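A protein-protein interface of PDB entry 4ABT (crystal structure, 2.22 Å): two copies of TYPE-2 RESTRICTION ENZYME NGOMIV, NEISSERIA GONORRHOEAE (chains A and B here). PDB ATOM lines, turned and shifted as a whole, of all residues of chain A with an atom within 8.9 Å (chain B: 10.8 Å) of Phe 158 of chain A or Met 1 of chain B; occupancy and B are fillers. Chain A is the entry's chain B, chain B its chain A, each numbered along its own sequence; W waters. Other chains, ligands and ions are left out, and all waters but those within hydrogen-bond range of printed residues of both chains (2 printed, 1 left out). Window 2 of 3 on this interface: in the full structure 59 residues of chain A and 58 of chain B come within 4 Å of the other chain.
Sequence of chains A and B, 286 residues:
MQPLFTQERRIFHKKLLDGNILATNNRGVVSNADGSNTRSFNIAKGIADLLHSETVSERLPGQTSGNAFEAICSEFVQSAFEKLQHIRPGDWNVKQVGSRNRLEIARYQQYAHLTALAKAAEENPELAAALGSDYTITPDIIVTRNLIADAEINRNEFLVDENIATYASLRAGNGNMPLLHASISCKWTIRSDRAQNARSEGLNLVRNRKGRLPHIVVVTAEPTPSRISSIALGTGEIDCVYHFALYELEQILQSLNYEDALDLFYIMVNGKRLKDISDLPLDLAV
Printed residues of chain A that touch a printed residue of chain B: Ile 153, Arg 155, Asn 156, Glu 157, Phe 158, Leu 159, Val 160, Asp 161 and Ile 164. Hydrophobic or aromatic side chains of chain A within 4 Å of the printed part of chain B: Phe 158, Leu 159, Val 160 and Ile 164. Among the printed residues, Asp or Glu carboxylates within 4 Å of a Lys or Arg side-chain nitrogen of the other chain: Glu 157 of chain A with Lys 83 of chain B (3.4 Å).
No residue of chain B comes within 4 Å of Asn 154 of chain A. Printed residues of chain B within 4 Å of Arg 155 of chain A: His 86. Of chain B, only Leu 4 (3.2 Å) and Lys 83 (3.4 Å) come within 4 Å of Glu 157 of chain A. Of chain B, only Pro 3, Leu 4, Phe 5, Lys 83 and Leu 84 come within 4 Å of Leu 159 of chain A. Of chain B, only Pro 3 and Phe 5 come within 4 Å of Val 160 of chain A. Arg 171 of chain A touches none of the printed residues of chain B. Printed residues of chain A within 4 Å of Gln 2 of chain B: Phe 158. The nearest printed residue of chain B that does not touch Asn 156 of chain A is Lys 83 of chain B (6.1 Å).
N of Phe 5 of chain B sits at hydrogen-bond distance from O of Leu 159 of chain A (3.1 Å). The backbone NH (N) of Leu 4 of chain B lies within hydrogen-bond range of the backbone carbonyl oxygen (O) of Leu 159 of chain A, 3.4 Å away. N of Leu 4 of chain B lies within hydrogen-bond range of O of Phe 158 of chain A (2.7 Å). The side-chain amino group (NZ) of Lys 83 of chain B is in salt-bridge range of the side-chain carboxylate (OE1) of Glu 157 of chain A (3.4 Å).
Water W1 lies within hydrogen-bond range of the side-chain hydroxyl of Thr 6 of chain B (2.5 Å) and the side-chain carboxylate of Asp 161 of chain A (2.6 Å). Water W2 bridges the side-chain carboxylate of Glu 157 of chain A (2.7 Å) and the backbone carbonyl oxygen of Lys 83 of chain B (2.7 Å).
No position is printed for both chains. Of the 20 pairs that touch across the chains among the printed residues, none has its exchanged pair printed and touching as well.
NE2 of Gln 7 of chain B is in hydrogen-bond range of O of Gln 2 of chain B (3.1 Å). OD1 of Asp 161 of chain A sits at hydrogen-bond distance from N of Asn 163 of chain A, at 3.0 Å. The side-chain amide oxygen (OD1) of Asn 154 of chain A sits at hydrogen-bond distance from the backbone NH (N) of Leu 159 of chain A (2.7 Å). A ring nitrogen (NE2) of His 86 of chain B is in hydrogen-bond range of the backbone carbonyl oxygen of Lys 83 of chain B. NH2 of Arg 171 of chain A sits at hydrogen-bond distance from O of Asp 161 of chain A, 2.8 Å away. The backbone carbonyl oxygen (O) of Ile 164 of chain A sits at hydrogen-bond distance from the guanidinium group (NH1) of Arg 171 of chain A (2.8 Å).
Among the printed residues, merely in contact across the chains: Ile 153 of chain A with His 86 of chain B (3.1 Å), Arg 155 of chain A with His 86 of chain B (3.6 Å), Asn 156 of chain A with His 86 of chain B (3.98 Å), Glu 157 of chain A with Leu 4 of chain B (3.2 Å), Phe 158 of chain A with Met 1 of chain B (3.8 Å), Phe 158 of chain A with Gln 2 of chain B (3.9 Å), Phe 158 of chain A with Pro 3 of chain B (3.3 Å), Leu 159 of chain A with Pro 3 of chain B (3.2 Å), Leu 159 of chain A with Lys 83 of chain B (3.8 Å), Leu 159 of chain A with Leu 84 of chain B (3.7 Å), Val 160 of chain A with Pro 3 of chain B (3.7 Å), Val 160 of chain A with Phe 5 of chain B (3.5 Å), Asp 161 of chain A with Pro 3 of chain B (3.4 Å), Ile 164 of chain A with Phe 5 of chain B (3.9 Å), Ile 164 of chain A with Thr 6 of chain B (3.3 Å) and Ile 164 of chain A with Arg 9 of chain B (3.6 Å).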
ATOM      1  N   ASP A 150     -24.659  15.394  34.688  1.00  0.00           N
ATOM      2  CA  ASP A 150     -24.963  15.292  33.270  1.00  0.00           C
ATOM      3  C   ASP A 150     -24.987  16.655  32.605  1.00  0.00           C
ATOM      4  O   ASP A 150     -24.546  16.776  31.465  1.00  0.00           O
ATOM      5  CB  ASP A 150     -26.343  14.611  33.023  1.00  0.00           C
ATOM      6  CG  ASP A 150     -26.326  13.084  33.259  1.00  0.00           C
ATOM      7  OD1 ASP A 150     -25.306  12.520  33.735  1.00  0.00           O
ATOM      8  OD2 ASP A 150     -27.365  12.455  32.998  1.00  0.00           O
ATOM      9  N   ALA A 151     -25.552  17.662  33.278  1.00  0.00           N
ATOM     10  CA  ALA A 151     -25.538  19.026  32.764  1.00  0.00           C
ATOM     11  C   ALA A 151     -24.146  19.487  32.371  1.00  0.00           C
ATOM     12  O   ALA A 151     -24.006  20.210  31.401  1.00  0.00           O
ATOM     13  CB  ALA A 151     -26.090  19.975  33.787  1.00  0.00           C
ATOM     14  N   ILE A 153     -21.452  17.201  31.853  1.00  0.00           N
ATOM     15  CA  ILE A 153     -21.080  16.294  30.767  1.00  0.00           C
ATOM     16  C   ILE A 153     -21.713  16.706  29.413  1.00  0.00           C
ATOM     17  O   ILE A 153     -21.035  16.705  28.382  1.00  0.00           O
ATOM     18  CB  ILE A 153     -21.370  14.853  31.128  1.00  0.00           C
ATOM     19  CG1 ILE A 153     -20.576  14.487  32.362  1.00  0.00           C
ATOM     20  CG2 ILE A 153     -20.978  13.923  30.006  1.00  0.00           C
ATOM     21  CD1 ILE A 153     -20.978  13.175  32.903  1.00  0.00           C
ATOM     22  N   ASN A 154     -22.979  17.103  29.453  1.00  0.00           N
ATOM     23  CA  ASN A 154     -23.750  17.396  28.278  1.00  0.00           C
ATOM     24  C   ASN A 154     -23.768  18.916  27.968  1.00  0.00           C
ATOM     25  O   ASN A 154     -24.736  19.442  27.419  1.00  0.00           O
ATOM     26  CB  ASN A 154     -25.190  16.849  28.447  1.00  0.00           C
ATOM     27  CG  ASN A 154     -25.257  15.337  28.425  1.00  0.00           C
ATOM     28  OD1 ASN A 154     -24.393  14.670  27.845  1.00  0.00           O
ATOM     29  ND2 ASN A 154     -26.320  14.785  29.003  1.00  0.00           N
ATOM     30  N   ARG A 155     -22.679  19.611  28.294  1.00  0.00           N
ATOM     31  CA  ARG A 155     -22.658  21.069  28.238  1.00  0.00           C
ATOM     32  C   ARG A 155     -22.882  21.630  26.820  1.00  0.00           C
ATOM     33  O   ARG A 155     -23.579  22.649  26.639  1.00  0.00           O
ATOM     34  CB  ARG A 155     -21.355  21.580  28.891  1.00  0.00           C
ATOM     35  CG  ARG A 155     -20.924  22.944  28.443  1.00  0.00           C
ATOM     36  CD  ARG A 155     -20.540  23.865  29.590  1.00  0.00           C
ATOM     37  NE  ARG A 155     -19.234  23.562  30.198  1.00  0.00           N
ATOM     38  CZ  ARG A 155     -18.042  23.943  29.725  1.00  0.00           C
ATOM     39  NH1 ARG A 155     -17.931  24.640  28.584  1.00  0.00           N
ATOM     40  NH2 ARG A 155     -16.941  23.605  30.391  1.00  0.00           N
ATOM     41  N   ASN A 156     -22.320  20.930  25.826  1.00  0.00           N
ATOM     42  CA  ASN A 156     -22.277  21.349  24.445  1.00  0.00           C
ATOM     43  C   ASN A 156     -22.947  20.326  23.537  1.00  0.00           C
ATOM     44  O   ASN A 156     -23.466  20.695  22.477  1.00  0.00           O
ATOM     45  CB  ASN A 156     -20.819  21.514  24.013  1.00  0.00           C
ATOM     46  CG  ASN A 156     -20.052  22.542  24.853  1.00  0.00           C
ATOM     47  OD1 ASN A 156     -20.544  23.647  25.187  1.00  0.00           O
ATOM     48  ND2 ASN A 156     -18.837  22.185  25.199  1.00  0.00           N
ATOM     49  N   GLU A 157     -22.964  19.058  23.956  1.00  0.00           N
ATOM     50  CA  GLU A 157     -23.626  17.942  23.216  1.00  0.00           C
ATOM     51  C   GLU A 157     -24.356  16.963  24.129  1.00  0.00           C
ATOM     52  O   GLU A 157     -24.057  16.821  25.320  1.00  0.00           O
ATOM     53  CB  GLU A 157     -22.603  17.166  22.400  1.00  0.00           C
ATOM     54  CG  GLU A 157     -21.860  18.057  21.453  1.00  0.00           C
ATOM     55  CD  GLU A 157     -20.727  17.388  20.815  1.00  0.00           C
ATOM     56  OE1 GLU A 157     -20.975  16.799  19.742  1.00  0.00           O
ATOM     57  OE2 GLU A 157     -19.591  17.464  21.344  1.00  0.00           O
ATOM     58  N   PHE A 158     -25.356  16.307  23.590  1.00  0.00           N
ATOM     59  CA  PHE A 158     -26.051  15.285  24.335  1.00  0.00           C
ATOM     60  C   PHE A 158     -25.206  13.983  24.270  1.00  0.00           C
ATOM     61  O   PHE A 158     -25.380  13.139  23.342  1.00  0.00           O
ATOM     62  CB  PHE A 158     -27.460  15.147  23.758  1.00  0.00           C
ATOM     63  CG  PHE A 158     -28.309  14.119  24.443  1.00  0.00           C
ATOM     64  CD1 PHE A 158     -28.435  14.094  25.811  1.00  0.00           C
ATOM     65  CD2 PHE A 158     -29.044  13.209  23.684  1.00  0.00           C
ATOM     66  CE1 PHE A 158     -29.243  13.150  26.419  1.00  0.00           C
ATOM     67  CE2 PHE A 158     -29.874  12.250  24.276  1.00  0.00           C
ATOM     68  CZ  PHE A 158     -29.978  12.215  25.642  1.00  0.00           C
ATOM     69  N   LEU A 159     -24.280  13.860  25.232  1.00  0.00           N
ATOM     70  CA  LEU A 159     -23.296  12.773  25.266  1.00  0.00           C
ATOM     71  C   LEU A 159     -23.842  11.561  25.963  1.00  0.00           C
ATOM     72  O   LEU A 159     -23.635  10.426  25.526  1.00  0.00           O
ATOM     73  CB  LEU A 159     -22.056  13.203  26.025  1.00  0.00           C
ATOM     74  CG  LEU A 159     -21.307  14.389  25.411  1.00  0.00           C
ATOM     75  CD1 LEU A 159     -19.969  14.569  26.133  1.00  0.00           C
ATOM     76  CD2 LEU A 159     -21.104  14.184  23.902  1.00  0.00           C
ATOM     77  N   VAL A 160     -24.535  11.795  27.065  1.00  0.00           N
ATOM     78  CA  VAL A 160     -24.962  10.695  27.901  1.00  0.00           C
ATOM     79  C   VAL A 160     -26.361  10.869  28.498  1.00  0.00           C
ATOM     80  O   VAL A 160     -26.897  11.986  28.565  1.00  0.00           O
ATOM     81  CB  VAL A 160     -23.975  10.444  29.060  1.00  0.00           C
ATOM     82  CG1 VAL A 160     -22.516  10.129  28.496  1.00  0.00           C
ATOM     83  CG2 VAL A 160     -24.012  11.603  30.089  1.00  0.00           C
ATOM     84  N   ASP A 161     -26.918   9.721  28.911  1.00  0.00           N
ATOM     85  CA  ASP A 161     -28.110   9.608  29.667  1.00  0.00           C
ATOM     86  C   ASP A 161     -27.900   8.482  30.684  1.00  0.00           C
ATOM     87  O   ASP A 161     -26.747   8.158  31.041  1.00  0.00           O
ATOM     88  CB  ASP A 161     -29.365   9.448  28.783  1.00  0.00           C
ATOM     89  CG  ASP A 161     -29.445   8.082  28.036  1.00  0.00           C
ATOM     90  OD1 ASP A 161     -28.611   7.152  28.262  1.00  0.00           O
ATOM     91  OD2 ASP A 161     -30.388   7.959  27.213  1.00  0.00           O
ATOM     92  N   GLU A 162     -29.002   7.940  31.207  1.00  0.00           N
ATOM     93  CA  GLU A 162     -28.898   7.131  32.404  1.00  0.00           C
ATOM     94  C   GLU A 162     -28.743   5.702  32.014  1.00  0.00           C
ATOM     95  O   GLU A 162     -28.714   4.856  32.877  1.00  0.00           O
ATOM     96  CB  GLU A 162     -30.105   7.301  33.337  1.00  0.00           C
ATOM     97  CG  GLU A 162     -31.404   6.656  32.824  1.00  0.00           C
ATOM     98  CD  GLU A 162     -32.208   7.568  31.889  1.00  0.00           C
ATOM     99  OE1 GLU A 162     -31.740   8.702  31.528  1.00  0.00           O
ATOM    100  OE2 GLU A 162     -33.333   7.148  31.557  1.00  0.00           O
ATOM    101  N   ASN A 163     -28.621   5.461  30.713  1.00  0.00           N
ATOM    102  CA  ASN A 163     -28.520   4.139  30.126  1.00  0.00           C
ATOM    103  C   ASN A 163     -27.208   3.881  29.384  1.00  0.00           C
ATOM    104  O   ASN A 163     -27.057   2.864  28.689  1.00  0.00           O
ATOM    105  CB  ASN A 163     -29.658   3.989  29.115  1.00  0.00           C
ATOM    106  CG  ASN A 163     -31.006   3.782  29.788  1.00  0.00           C
ATOM    107  OD1 ASN A 163     -31.102   3.065  30.776  1.00  0.00           O
ATOM    108  ND2 ASN A 163     -32.045   4.409  29.252  1.00  0.00           N
ATOM    109  N   ILE A 164     -26.265   4.804  29.507  1.00  0.00           N
ATOM    110  CA  ILE A 164     -24.964   4.671  28.834  1.00  0.00           C
ATOM    111  C   ILE A 164     -23.886   5.130  29.805  1.00  0.00           C
ATOM    112  O   ILE A 164     -24.144   6.031  30.594  1.00  0.00           O
ATOM    113  CB  ILE A 164     -24.944   5.503  27.521  1.00  0.00           C
ATOM    114  CG1 ILE A 164     -23.762   5.087  26.649  1.00  0.00           C
ATOM    115  CG2 ILE A 164     -25.055   7.028  27.763  1.00  0.00           C
ATOM    116  CD1 ILE A 164     -23.871   3.659  26.198  1.00  0.00           C
ATOM    117  N   ARG A 171     -19.121  10.465  37.157  1.00  0.00           N
ATOM    118  CA  ARG A 171     -20.570  10.695  37.140  1.00  0.00           C
ATOM    119  C   ARG A 171     -21.162  10.673  38.500  1.00  0.00           C
ATOM    120  O   ARG A 171     -21.057   9.678  39.215  1.00  0.00           O
ATOM    121  CB  ARG A 171     -21.303   9.724  36.239  1.00  0.00           C
ATOM    122  CG  ARG A 171     -21.148  10.139  34.813  1.00  0.00           C
ATOM    123  CD  ARG A 171     -22.025   9.301  33.963  1.00  0.00           C
ATOM    124  NE  ARG A 171     -23.353   9.890  33.774  1.00  0.00           N
ATOM    125  CZ  ARG A 171     -24.252   9.299  33.021  1.00  0.00           C
ATOM    126  NH1 ARG A 171     -23.936   8.146  32.447  1.00  0.00           N
ATOM    127  NH2 ARG A 171     -25.433   9.846  32.835  1.00  0.00           N
ATOM    128  N   MET B   1     -32.646  11.870  18.918  1.00  0.00           N
ATOM    129  CA  MET B   1     -31.370  11.089  18.813  1.00  0.00           C
ATOM    130  C   MET B   1     -31.061  10.284  20.092  1.00  0.00           C
ATOM    131  O   MET B   1     -31.519  10.628  21.203  1.00  0.00           O
ATOM    132  CB  MET B   1     -30.219  12.081  18.627  1.00  0.00           C
ATOM    133  CG  MET B   1     -30.174  13.100  19.762  1.00  0.00           C
ATOM    134  SD  MET B   1     -28.935  14.388  19.521  1.00  0.00           S
ATOM    135  CE  MET B   1     -27.478  13.431  19.985  1.00  0.00           C
ATOM    136  N   GLN B   2     -30.229   9.266  19.941  1.00  0.00           N
ATOM    137  CA  GLN B   2     -29.549   8.693  21.097  1.00  0.00           C
ATOM    138  C   GLN B   2     -28.492   9.681  21.615  1.00  0.00           C
ATOM    139  O   GLN B   2     -28.004  10.525  20.831  1.00  0.00           O
ATOM    140  CB  GLN B   2     -28.824   7.400  20.706  1.00  0.00           C
ATOM    141  CG  GLN B   2     -29.686   6.322  20.088  1.00  0.00           C
ATOM    142  CD  GLN B   2     -30.467   5.585  21.099  1.00  0.00           C
ATOM    143  OE1 GLN B   2     -31.011   6.191  22.037  1.00  0.00           O
ATOM    144  NE2 GLN B   2     -30.525   4.251  20.955  1.00  0.00           N
ATOM    145  N   PRO B   3     -28.105   9.556  22.898  1.00  0.00           N
ATOM    146  CA  PRO B   3     -26.918  10.245  23.325  1.00  0.00           C
ATOM    147  C   PRO B   3     -25.746   9.824  22.457  1.00  0.00           C
ATOM    148  O   PRO B   3     -25.743   8.713  21.906  1.00  0.00           O
ATOM    149  CB  PRO B   3     -26.700   9.726  24.733  1.00  0.00           C
ATOM    150  CG  PRO B   3     -27.966   9.115  25.186  1.00  0.00           C
ATOM    151  CD  PRO B   3     -28.651   8.683  23.950  1.00  0.00           C
ATOM    152  N   LEU B   4     -24.754  10.694  22.310  1.00  0.00           N
ATOM    153  CA  LEU B   4     -23.691  10.411  21.354  1.00  0.00           C
ATOM    154  C   LEU B   4     -22.859   9.193  21.733  1.00  0.00           C
ATOM    155  O   LEU B   4     -22.413   8.450  20.849  1.00  0.00           O
ATOM    156  CB  LEU B   4     -22.775  11.634  21.164  1.00  0.00           C
ATOM    157  CG  LEU B   4     -23.348  12.834  20.374  1.00  0.00           C
ATOM    158  CD1 LEU B   4     -22.239  13.865  20.167  1.00  0.00           C
ATOM    159  CD2 LEU B   4     -23.954  12.471  18.993  1.00  0.00           C
ATOM    160  N   PHE B   5     -22.647   8.979  23.025  1.00  0.00           N
ATOM    161  CA  PHE B   5     -21.870   7.807  23.468  1.00  0.00           C
ATOM    162  C   PHE B   5     -22.590   6.485  23.208  1.00  0.00           C
ATOM    163  O   PHE B   5     -21.951   5.448  22.988  1.00  0.00           O
ATOM    164  CB  PHE B   5     -21.411   7.926  24.930  1.00  0.00           C
ATOM    165  CG  PHE B   5     -20.285   8.927  25.145  1.00  0.00           C
ATOM    166  CD1 PHE B   5     -19.691   9.572  24.074  1.00  0.00           C
ATOM    167  CD2 PHE B   5     -19.816   9.184  26.422  1.00  0.00           C
ATOM    168  CE1 PHE B   5     -18.622  10.503  24.282  1.00  0.00           C
ATOM    169  CE2 PHE B   5     -18.769  10.107  26.664  1.00  0.00           C
ATOM    170  CZ  PHE B   5     -18.174  10.789  25.591  1.00  0.00           C
ATOM    171  N   THR B   6     -23.916   6.530  23.191  1.00  0.00           N
ATOM    172  CA  THR B   6     -24.695   5.356  22.840  1.00  0.00           C
ATOM    173  C   THR B   6     -24.533   5.098  21.356  1.00  0.00           C
ATOM    174  O   THR B   6     -24.325   3.984  20.958  1.00  0.00           O
ATOM    175  CB  THR B   6     -26.182   5.526  23.156  1.00  0.00           C
ATOM    176  OG1 THR B   6     -26.386   5.618  24.563  1.00  0.00           O
ATOM    177  CG2 THR B   6     -27.002   4.298  22.653  1.00  0.00           C
ATOM    178  N   GLN B   7     -24.623   6.131  20.527  1.00  0.00           N
ATOM    179  CA  GLN B   7     -24.299   5.999  19.083  1.00  0.00           C
ATOM    180  C   GLN B   7     -22.881   5.476  18.827  1.00  0.00           C
ATOM    181  O   GLN B   7     -22.666   4.637  17.937  1.00  0.00           O
ATOM    182  CB  GLN B   7     -24.472   7.347  18.391  1.00  0.00           C
ATOM    183  CG  GLN B   7     -25.924   7.739  18.164  1.00  0.00           C
ATOM    184  CD  GLN B   7     -26.045   9.061  17.420  1.00  0.00           C
ATOM    185  OE1 GLN B   7     -25.537   9.201  16.297  1.00  0.00           O
ATOM    186  NE2 GLN B   7     -26.729  10.052  18.043  1.00  0.00           N
ATOM    187  N   GLU B   8     -21.902   5.958  19.601  1.00  0.00           N
ATOM    188  CA  GLU B   8     -20.521   5.510  19.410  1.00  0.00           C
ATOM    189  C   GLU B   8     -20.430   4.026  19.776  1.00  0.00           C
ATOM    190  O   GLU B   8     -19.782   3.257  19.082  1.00  0.00           O
ATOM    191  CB  GLU B   8     -19.527   6.303  20.231  1.00  0.00           C
ATOM    192  CG  GLU B   8     -19.347   7.748  19.810  1.00  0.00           C
ATOM    193  CD  GLU B   8     -18.425   7.961  18.631  1.00  0.00           C
ATOM    194  OE1 GLU B   8     -17.924   6.996  18.001  1.00  0.00           O
ATOM    195  OE2 GLU B   8     -18.195   9.146  18.332  1.00  0.00           O
ATOM    196  N   ARG B   9     -21.164   3.625  20.810  1.00  0.00           N
ATOM    197  CA  ARG B   9     -21.083   2.257  21.274  1.00  0.00           C
ATOM    198  C   ARG B   9     -21.625   1.347  20.208  1.00  0.00           C
ATOM    199  O   ARG B   9     -21.010   0.329  19.930  1.00  0.00           O
ATOM    200  CB  ARG B   9     -21.786   2.086  22.626  1.00  0.00           C
ATOM    201  CG  ARG B   9     -21.956   0.656  23.137  1.00  0.00           C
ATOM    202  CD  ARG B   9     -22.645   0.741  24.524  1.00  0.00           C
ATOM    203  NE  ARG B   9     -22.359  -0.424  25.353  1.00  0.00           N
ATOM    204  CZ  ARG B   9     -23.024  -1.579  25.299  1.00  0.00           C
ATOM    205  NH1 ARG B   9     -24.037  -1.755  24.428  1.00  0.00           N
ATOM    206  NH2 ARG B   9     -22.674  -2.582  26.114  1.00  0.00           N
ATOM    207  N   ALA B  80     -14.848   9.163  20.789  1.00  0.00           N
ATOM    208  CA  ALA B  80     -15.624   9.497  21.974  1.00  0.00           C
ATOM    209  C   ALA B  80     -14.900  10.470  22.935  1.00  0.00           C
ATOM    210  O   ALA B  80     -15.496  11.411  23.398  1.00  0.00           O
ATOM    211  CB  ALA B  80     -16.042   8.271  22.656  1.00  0.00           C
ATOM    212  N   LYS B  83     -15.037  14.333  22.396  1.00  0.00           N
ATOM    213  CA  LYS B  83     -16.216  15.052  22.870  1.00  0.00           C
ATOM    214  C   LYS B  83     -16.059  15.650  24.261  1.00  0.00           C
ATOM    215  O   LYS B  83     -16.945  16.369  24.700  1.00  0.00           O
ATOM    216  CB  LYS B  83     -17.460  14.138  22.877  1.00  0.00           C
ATOM    217  CG  LYS B  83     -17.829  13.481  21.495  1.00  0.00           C
ATOM    218  CD  LYS B  83     -17.869  14.523  20.406  1.00  0.00           C
ATOM    219  CE  LYS B  83     -18.434  13.978  19.101  1.00  0.00           C
ATOM    220  NZ  LYS B  83     -18.555  15.119  18.105  1.00  0.00           N
ATOM    221  N   LEU B  84     -14.958  15.338  24.946  1.00  0.00           N
ATOM    222  CA  LEU B  84     -14.768  15.646  26.391  1.00  0.00           C
ATOM    223  C   LEU B  84     -13.758  16.788  26.672  1.00  0.00           C
ATOM    224  O   LEU B  84     -13.161  16.872  27.762  1.00  0.00           O
ATOM    225  CB  LEU B  84     -14.400  14.358  27.141  1.00  0.00           C
ATOM    226  CG  LEU B  84     -15.450  13.231  27.135  1.00  0.00           C
ATOM    227  CD1 LEU B  84     -14.990  11.969  27.927  1.00  0.00           C
ATOM    228  CD2 LEU B  84     -16.735  13.771  27.690  1.00  0.00           C
ATOM    229  N   HIS B  86     -14.118  19.890  27.174  1.00  0.00           N
ATOM    230  CA  HIS B  86     -14.562  20.807  28.185  1.00  0.00           C
ATOM    231  C   HIS B  86     -14.357  20.226  29.583  1.00  0.00           C
ATOM    232  O   HIS B  86     -14.249  20.975  30.566  1.00  0.00           O
ATOM    233  CB  HIS B  86     -16.033  21.143  27.935  1.00  0.00           C
ATOM    234  CG  HIS B  86     -16.920  19.929  27.857  1.00  0.00           C
ATOM    235  ND1 HIS B  86     -17.880  19.651  28.800  1.00  0.00           N
ATOM    236  CD2 HIS B  86     -16.966  18.913  26.968  1.00  0.00           C
ATOM    237  CE1 HIS B  86     -18.496  18.531  28.479  1.00  0.00           C
ATOM    238  NE2 HIS B  86     -17.954  18.065  27.378  1.00  0.00           N
ATOM    239  N   LEU B 282     -15.097   8.594  29.363  1.00  0.00           N
ATOM    240  CA  LEU B 282     -15.163   9.395  30.598  1.00  0.00           C
ATOM    241  C   LEU B 282     -14.142   9.009  31.654  1.00  0.00           C
ATOM    242  O   LEU B 282     -13.648   9.880  32.360  1.00  0.00           O
ATOM    243  CB  LEU B 282     -16.539   9.345  31.224  1.00  0.00           C
ATOM    244  CG  LEU B 282     -17.491  10.338  30.606  1.00  0.00           C
ATOM    245  CD1 LEU B 282     -18.933   9.809  30.813  1.00  0.00           C
ATOM    246  CD2 LEU B 282     -17.268  11.688  31.296  1.00  0.00           C
HETATM  247  O   HOH W   1     -28.311   5.725  26.103  1.00  0.00           O
HETATM  248  O   HOH W   2     -19.165  17.712  23.957  1.00  0.00           O
